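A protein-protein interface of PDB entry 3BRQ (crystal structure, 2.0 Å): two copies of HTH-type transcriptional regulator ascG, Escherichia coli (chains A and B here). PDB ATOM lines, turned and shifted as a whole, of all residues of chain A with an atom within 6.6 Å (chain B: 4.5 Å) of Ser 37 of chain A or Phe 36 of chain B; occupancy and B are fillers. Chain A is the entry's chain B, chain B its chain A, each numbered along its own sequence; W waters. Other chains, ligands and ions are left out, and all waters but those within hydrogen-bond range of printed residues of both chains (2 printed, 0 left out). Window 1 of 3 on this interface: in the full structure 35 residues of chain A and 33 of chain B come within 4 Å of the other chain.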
ATOM      1  N   ILE A  34     -16.383 -18.142   7.675  1.00  0.00           N
ATOM      2  CA  ILE A  34     -15.343 -17.307   8.255  1.00  0.00           C
ATOM      3  C   ILE A  34     -16.078 -16.408   9.275  1.00  0.00           C
ATOM      4  O   ILE A  34     -16.883 -15.550   8.893  1.00  0.00           O
ATOM      5  CB  ILE A  34     -14.617 -16.411   7.179  1.00  0.00           C
ATOM      6  CG1 ILE A  34     -14.172 -17.206   5.928  1.00  0.00           C
ATOM      7  CG2 ILE A  34     -13.489 -15.548   7.837  1.00  0.00           C
ATOM      8  CD1 ILE A  34     -13.325 -18.440   6.191  1.00  0.00           C
ATOM      9  N   TYR A  35     -15.841 -16.606  10.561  1.00  0.00           N
ATOM     10  CA  TYR A  35     -16.640 -15.858  11.574  1.00  0.00           C
ATOM     11  C   TYR A  35     -16.750 -14.372  11.202  1.00  0.00           C
ATOM     12  O   TYR A  35     -15.755 -13.701  10.951  1.00  0.00           O
ATOM     13  CB  TYR A  35     -16.068 -16.055  12.984  1.00  0.00           C
ATOM     14  CG  TYR A  35     -16.834 -15.362  14.122  1.00  0.00           C
ATOM     15  CD1 TYR A  35     -18.193 -15.076  14.030  1.00  0.00           C
ATOM     16  CD2 TYR A  35     -16.184 -15.046  15.316  1.00  0.00           C
ATOM     17  CE1 TYR A  35     -18.894 -14.450  15.099  1.00  0.00           C
ATOM     18  CE2 TYR A  35     -16.860 -14.435  16.376  1.00  0.00           C
ATOM     19  CZ  TYR A  35     -18.207 -14.143  16.266  1.00  0.00           C
ATOM     20  OH  TYR A  35     -18.844 -13.538  17.333  1.00  0.00           O
ATOM     21  N   PHE A  36     -17.973 -13.875  11.098  1.00  0.00           N
ATOM     22  CA  PHE A  36     -18.194 -12.564  10.504  1.00  0.00           C
ATOM     23  C   PHE A  36     -17.768 -11.407  11.453  1.00  0.00           C
ATOM     24  O   PHE A  36     -17.127 -10.445  11.028  1.00  0.00           O
ATOM     25  CB  PHE A  36     -19.648 -12.534  10.006  1.00  0.00           C
ATOM     26  CG  PHE A  36     -20.102 -11.251   9.347  1.00  0.00           C
ATOM     27  CD1 PHE A  36     -19.220 -10.228   8.998  1.00  0.00           C
ATOM     28  CD2 PHE A  36     -21.451 -11.107   9.017  1.00  0.00           C
ATOM     29  CE1 PHE A  36     -19.681  -9.057   8.417  1.00  0.00           C
ATOM     30  CE2 PHE A  36     -21.933  -9.929   8.405  1.00  0.00           C
ATOM     31  CZ  PHE A  36     -21.036  -8.905   8.105  1.00  0.00           C
ATOM     32  N   SER A  37     -18.070 -11.480  12.732  1.00  0.00           N
ATOM     33  CA  SER A  37     -17.699 -10.314  13.546  1.00  0.00           C
ATOM     34  C   SER A  37     -16.164 -10.275  13.700  1.00  0.00           C
ATOM     35  O   SER A  37     -15.569  -9.189  13.671  1.00  0.00           O
ATOM     36  CB  SER A  37     -18.407 -10.327  14.880  1.00  0.00           C
ATOM     37  OG  SER A  37     -17.891 -11.388  15.618  1.00  0.00           O
ATOM     38  N   GLU A  38     -15.546 -11.458  13.787  1.00  0.00           N
ATOM     39  CA  GLU A  38     -14.089 -11.585  13.765  1.00  0.00           C
ATOM     40  C   GLU A  38     -13.489 -11.048  12.475  1.00  0.00           C
ATOM     41  O   GLU A  38     -12.547 -10.251  12.523  1.00  0.00           O
ATOM     42  CB  GLU A  38     -13.651 -13.028  13.951  1.00  0.00           C
ATOM     43  CG  GLU A  38     -12.405 -13.169  14.835  1.00  0.00           C
ATOM     44  CD  GLU A  38     -11.662 -14.494  14.611  1.00  0.00           C
ATOM     45  OE1 GLU A  38     -12.327 -15.516  14.275  1.00  0.00           O
ATOM     46  OE2 GLU A  38     -10.411 -14.521  14.758  1.00  0.00           O
ATOM     47  N   LEU A  39     -14.046 -11.442  11.323  1.00  0.00           N
ATOM     48  CA  LEU A  39     -13.489 -10.979  10.072  1.00  0.00           C
ATOM     49  C   LEU A  39     -13.653  -9.465   9.951  1.00  0.00           C
ATOM     50  O   LEU A  39     -12.752  -8.781   9.491  1.00  0.00           O
ATOM     51  CB  LEU A  39     -14.063 -11.751   8.843  1.00  0.00           C
ATOM     52  CG  LEU A  39     -15.291 -11.371   8.022  1.00  0.00           C
ATOM     53  CD1 LEU A  39     -15.026 -10.248   7.045  1.00  0.00           C
ATOM     54  CD2 LEU A  39     -15.735 -12.602   7.179  1.00  0.00           C
ATOM     55  N   LEU A  40     -14.792  -8.940  10.403  1.00  0.00           N
ATOM     56  CA  LEU A  40     -15.073  -7.512  10.260  1.00  0.00           C
ATOM     57  C   LEU A  40     -14.151  -6.716  11.174  1.00  0.00           C
ATOM     58  O   LEU A  40     -13.664  -5.648  10.823  1.00  0.00           O
ATOM     59  CB  LEU A  40     -16.538  -7.205  10.587  1.00  0.00           C
ATOM     60  CG  LEU A  40     -17.076  -5.788  10.344  1.00  0.00           C
ATOM     61  CD1 LEU A  40     -16.879  -5.320   8.888  1.00  0.00           C
ATOM     62  CD2 LEU A  40     -18.534  -5.685  10.710  1.00  0.00           C
ATOM     63  N   PHE A  41     -13.919  -7.268  12.347  1.00  0.00           N
ATOM     64  CA  PHE A  41     -13.065  -6.623  13.340  1.00  0.00           C
ATOM     65  C   PHE A  41     -11.662  -6.453  12.794  1.00  0.00           C
ATOM     66  O   PHE A  41     -11.077  -5.374  12.896  1.00  0.00           O
ATOM     67  CB  PHE A  41     -13.015  -7.429  14.634  1.00  0.00           C
ATOM     68  CG  PHE A  41     -12.056  -6.845  15.652  1.00  0.00           C
ATOM     69  CD1 PHE A  41     -12.276  -5.573  16.168  1.00  0.00           C
ATOM     70  CD2 PHE A  41     -10.907  -7.540  16.025  1.00  0.00           C
ATOM     71  CE1 PHE A  41     -11.380  -4.984  17.095  1.00  0.00           C
ATOM     72  CE2 PHE A  41      -9.990  -6.970  16.933  1.00  0.00           C
ATOM     73  CZ  PHE A  41     -10.245  -5.673  17.485  1.00  0.00           C
ATOM     74  N   HIS A  42     -11.121  -7.513  12.190  1.00  0.00           N
ATOM     75  CA  HIS A  42      -9.760  -7.439  11.680  1.00  0.00           C
ATOM     76  C   HIS A  42      -9.654  -6.654  10.385  1.00  0.00           C
ATOM     77  O   HIS A  42      -8.667  -5.968  10.173  1.00  0.00           O
ATOM     78  CB  HIS A  42      -9.127  -8.823  11.545  1.00  0.00           C
ATOM     79  CG  HIS A  42      -8.927  -9.508  12.856  1.00  0.00           C
ATOM     80  ND1 HIS A  42      -7.950  -9.127  13.748  1.00  0.00           N
ATOM     81  CD2 HIS A  42      -9.591 -10.535  13.437  1.00  0.00           C
ATOM     82  CE1 HIS A  42      -8.020  -9.891  14.826  1.00  0.00           C
ATOM     83  NE2 HIS A  42      -9.009 -10.753  14.659  1.00  0.00           N
ATOM     84  N   LEU A  56     -19.099  -1.360   4.582  1.00  0.00           N
ATOM     85  CA  LEU A  56     -19.618  -2.742   4.363  1.00  0.00           C
ATOM     86  C   LEU A  56     -21.024  -2.644   3.786  1.00  0.00           C
ATOM     87  O   LEU A  56     -21.873  -2.030   4.389  1.00  0.00           O
ATOM     88  CB  LEU A  56     -19.690  -3.495   5.688  1.00  0.00           C
ATOM     89  CG  LEU A  56     -20.471  -4.791   5.794  1.00  0.00           C
ATOM     90  CD1 LEU A  56     -19.733  -5.917   5.099  1.00  0.00           C
ATOM     91  CD2 LEU A  56     -20.616  -5.135   7.284  1.00  0.00           C
ATOM     92  N   VAL B  26     -21.057   2.034  13.453  1.00  0.00           N
ATOM     93  CA  VAL B  26     -20.694   1.285  14.658  1.00  0.00           C
ATOM     94  C   VAL B  26     -19.166   1.202  14.697  1.00  0.00           C
ATOM     95  O   VAL B  26     -18.513   0.646  13.772  1.00  0.00           O
ATOM     96  CB  VAL B  26     -21.266  -0.133  14.730  1.00  0.00           C
ATOM     97  CG1 VAL B  26     -20.966  -0.779  16.080  1.00  0.00           C
ATOM     98  CG2 VAL B  26     -22.770  -0.213  14.396  1.00  0.00           C
ATOM     99  N   LEU B  30     -16.777  -2.323  19.126  1.00  0.00           N
ATOM    100  CA  LEU B  30     -17.981  -3.144  19.413  1.00  0.00           C
ATOM    101  C   LEU B  30     -18.146  -4.362  18.481  1.00  0.00           C
ATOM    102  O   LEU B  30     -19.147  -5.116  18.604  1.00  0.00           O
ATOM    103  CB  LEU B  30     -19.265  -2.292  19.376  1.00  0.00           C
ATOM    104  CG  LEU B  30     -19.295  -1.142  20.401  1.00  0.00           C
ATOM    105  CD1 LEU B  30     -20.456  -0.202  20.081  1.00  0.00           C
ATOM    106  CD2 LEU B  30     -19.413  -1.688  21.794  1.00  0.00           C
ATOM    107  N   TYR B  31     -17.175  -4.589  17.588  1.00  0.00           N
ATOM    108  CA  TYR B  31     -17.283  -5.762  16.674  1.00  0.00           C
ATOM    109  C   TYR B  31     -16.801  -7.012  17.405  1.00  0.00           C
ATOM    110  O   TYR B  31     -15.790  -7.633  17.034  1.00  0.00           O
ATOM    111  CB  TYR B  31     -16.472  -5.561  15.397  1.00  0.00           C
ATOM    112  CG  TYR B  31     -16.843  -4.370  14.556  1.00  0.00           C
ATOM    113  CD1 TYR B  31     -17.849  -3.452  14.952  1.00  0.00           C
ATOM    114  CD2 TYR B  31     -16.142  -4.120  13.359  1.00  0.00           C
ATOM    115  CE1 TYR B  31     -18.149  -2.321  14.153  1.00  0.00           C
ATOM    116  CE2 TYR B  31     -16.451  -3.021  12.545  1.00  0.00           C
ATOM    117  CZ  TYR B  31     -17.447  -2.125  12.932  1.00  0.00           C
ATOM    118  OH  TYR B  31     -17.728  -1.042  12.099  1.00  0.00           O
ATOM    119  N   HIS B  32     -17.508  -7.318  18.488  1.00  0.00           N
ATOM    120  CA  HIS B  32     -17.311  -8.515  19.309  1.00  0.00           C
ATOM    121  C   HIS B  32     -18.679  -8.804  19.950  1.00  0.00           C
ATOM    122  O   HIS B  32     -18.926  -9.940  20.340  1.00  0.00           O
ATOM    123  CB  HIS B  32     -16.240  -8.324  20.417  1.00  0.00           C
ATOM    124  CG  HIS B  32     -14.993  -7.613  19.955  1.00  0.00           C
ATOM    125  ND1 HIS B  32     -13.941  -8.264  19.329  1.00  0.00           N
ATOM    126  CD2 HIS B  32     -14.644  -6.299  20.010  1.00  0.00           C
ATOM    127  CE1 HIS B  32     -13.007  -7.384  19.014  1.00  0.00           C
ATOM    128  NE2 HIS B  32     -13.410  -6.184  19.411  1.00  0.00           N
ATOM    129  N   TYR B  35     -23.969 -10.142  20.456  1.00  0.00           N
ATOM    130  CA  TYR B  35     -24.752  -8.927  20.322  1.00  0.00           C
ATOM    131  C   TYR B  35     -24.484  -8.171  19.004  1.00  0.00           C
ATOM    132  O   TYR B  35     -25.415  -7.691  18.339  1.00  0.00           O
ATOM    133  CB  TYR B  35     -24.492  -7.984  21.488  1.00  0.00           C
ATOM    134  CG  TYR B  35     -25.368  -6.768  21.406  1.00  0.00           C
ATOM    135  CD1 TYR B  35     -26.632  -6.776  21.953  1.00  0.00           C
ATOM    136  CD2 TYR B  35     -24.942  -5.614  20.750  1.00  0.00           C
ATOM    137  CE1 TYR B  35     -27.460  -5.674  21.854  1.00  0.00           C
ATOM    138  CE2 TYR B  35     -25.755  -4.503  20.664  1.00  0.00           C
ATOM    139  CZ  TYR B  35     -27.017  -4.541  21.216  1.00  0.00           C
ATOM    140  OH  TYR B  35     -27.848  -3.438  21.141  1.00  0.00           O
ATOM    141  N   PHE B  36     -23.209  -8.006  18.669  1.00  0.00           N
ATOM    142  CA  PHE B  36     -22.874  -7.383  17.395  1.00  0.00           C
ATOM    143  C   PHE B  36     -23.258  -8.288  16.210  1.00  0.00           C
ATOM    144  O   PHE B  36     -23.777  -7.834  15.179  1.00  0.00           O
ATOM    145  CB  PHE B  36     -21.396  -7.038  17.317  1.00  0.00           C
ATOM    146  CG  PHE B  36     -21.017  -6.446  16.005  1.00  0.00           C
ATOM    147  CD1 PHE B  36     -21.438  -5.165  15.659  1.00  0.00           C
ATOM    148  CD2 PHE B  36     -20.323  -7.208  15.062  1.00  0.00           C
ATOM    149  CE1 PHE B  36     -21.102  -4.604  14.411  1.00  0.00           C
ATOM    150  CE2 PHE B  36     -19.991  -6.656  13.832  1.00  0.00           C
ATOM    151  CZ  PHE B  36     -20.384  -5.346  13.526  1.00  0.00           C
ATOM    152  N   SER B  37     -22.934  -9.560  16.357  1.00  0.00           N
ATOM    153  CA  SER B  37     -23.308 -10.568  15.382  1.00  0.00           C
ATOM    154  C   SER B  37     -24.820 -10.473  15.072  1.00  0.00           C
ATOM    155  O   SER B  37     -25.208 -10.546  13.884  1.00  0.00           O
ATOM    156  CB  SER B  37     -22.973 -11.942  15.951  1.00  0.00           C
ATOM    157  OG  SER B  37     -23.706 -12.149  17.166  1.00  0.00           O
ATOM    158  N   GLU B  38     -25.626 -10.281  16.145  1.00  0.00           N
ATOM    159  CA  GLU B  38     -27.105 -10.238  16.135  1.00  0.00           C
ATOM    160  C   GLU B  38     -27.555  -9.005  15.402  1.00  0.00           C
ATOM    161  O   GLU B  38     -28.317  -9.097  14.420  1.00  0.00           O
ATOM    162  CB  GLU B  38     -27.722 -10.198  17.561  1.00  0.00           C
ATOM    163  CG  GLU B  38     -28.309 -11.531  18.136  1.00  0.00           C
ATOM    164  CD  GLU B  38     -29.640 -11.342  18.977  1.00  0.00           C
ATOM    165  OE1 GLU B  38     -29.591 -11.344  20.254  1.00  0.00           O
ATOM    166  OE2 GLU B  38     -30.740 -11.194  18.359  1.00  0.00           O
ATOM    167  N   LEU B  39     -27.108  -7.850  15.902  1.00  0.00           N
ATOM    168  CA  LEU B  39     -27.397  -6.582  15.290  1.00  0.00           C
ATOM    169  C   LEU B  39     -27.126  -6.581  13.789  1.00  0.00           C
ATOM    170  O   LEU B  39     -27.954  -6.141  13.045  1.00  0.00           O
ATOM    171  CB  LEU B  39     -26.595  -5.453  15.958  1.00  0.00           C
ATOM    172  CG  LEU B  39     -26.349  -4.220  15.065  1.00  0.00           C
ATOM    173  CD1 LEU B  39     -27.603  -3.438  14.780  1.00  0.00           C
ATOM    174  CD2 LEU B  39     -25.325  -3.309  15.683  1.00  0.00           C
ATOM    175  N   LEU B  40     -25.970  -7.053  13.346  1.00  0.00           N
ATOM    176  CA  LEU B  40     -25.698  -7.014  11.919  1.00  0.00           C
ATOM    177  C   LEU B  40     -26.667  -7.915  11.157  1.00  0.00           C
ATOM    178  O   LEU B  40     -27.276  -7.480  10.192  1.00  0.00           O
ATOM    179  CB  LEU B  40     -24.263  -7.369  11.598  1.00  0.00           C
ATOM    180  CG  LEU B  40     -23.790  -6.194  10.748  1.00  0.00           C
ATOM    181  CD1 LEU B  40     -22.427  -5.742  11.193  1.00  0.00           C
ATOM    182  CD2 LEU B  40     -23.863  -6.470   9.249  1.00  0.00           C
HETATM  183  O   HOH W   1     -21.439 -13.589  18.526  1.00  0.00           O
HETATM  184  O   HOH W   2     -18.035 -11.678  18.923  1.00  0.00           O
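Leu 40 of chain B touches Phe 36 of chain A. Ser 37 of chain A touches Tyr 31 of chain B. Phe 36 of chain B touches Ser 37 of chain A (CD2 to CB, 3.7 Å). Leu 40 of chain A touches Tyr 31 of chain B (CG to CD2, 3.6 Å). Leu 40 of chain A touches Phe 36 of chain B (CD2 to CZ, 3.4 Å). Leu 40 of chain A touches Leu 40 of chain B. Tyr 31 of chain B touches Phe 41 of chain A. NE2 of His 32 of chain B touches CE1 of Phe 41 of chain A, at 3.3 Å.
O of Val 26 of chain B lies within hydrogen-bond range of OH of Tyr 31 of chain B (2.5 Å). OG of Ser 37 of chain A lies close to OH of Tyr 35 of chain A (2.9 Å).
Water W2 lies within hydrogen-bond range of the backbone carbonyl oxygen of His 32 of chain B (2.4 Å), the side-chain hydroxyl of Tyr 35 of chain A (2.6 Å) and the side-chain hydroxyl of Ser 37 of chain A (3.3 Å). Water W1 lies within hydrogen-bond range of OH of Tyr 35 of chain A (2.9 Å) and OG of Ser 37 of chain B (3.0 Å).
Of the 10 printed residues of chain A, 4 touch a printed residue of chain B. Hydrophobic or aromatic side chains of chain A that line the printed part of chain B: Phe 36, Leu 40 and Phe 41. Hydrophobic or aromatic side chains of chain B within 4 Å of the printed part of chain A: Tyr 31, His 32, Phe 36 and Leu 40. Among the printed residues, 8 pairs touch across the chains.
Phe 36 of chain A touches Leu 40 of chain B, and with the chains exchanged Leu 40 of chain A touches Phe 36 of chain B. Ser 37 of chain A touches Phe 36 of chain B, but with the chains exchanged Phe 36 of chain A does not touch Ser 37 of chain B (6.2 Å). Leu 40 of chain A touches its own counterpart, Leu 40 of chain B.
Printed residues of chain B within 4 Å of Phe 36 of chain A: Leu 40 (3.9 Å). Ser 37 of chain A touches just these residues of chain B: Tyr 31 and Phe 36. Of the printed residues of chain B, Leu 40 of chain A touches Tyr 31 (3.6 Å), Phe 36 (3.4 Å) and Leu 40 (3.9 Å). His 42 of chain A touches none of the printed residues of chain B. Of the printed residues of chain A, His 32 of chain B touches Phe 41 (3.3 Å). Of chain A, only Ser 37 and Leu 40 come within 4 Å of Phe 36 of chain B. Ser 37 of chain B touches none of the printed residues of chain A. Printed residues of chain A within 4 Å of Leu 40 of chain B: Phe 36 and Leu 40. The nearest printed residue of chain B that does not touch Ser 37 of chain A is His 32 of chain B (4.7 Å).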
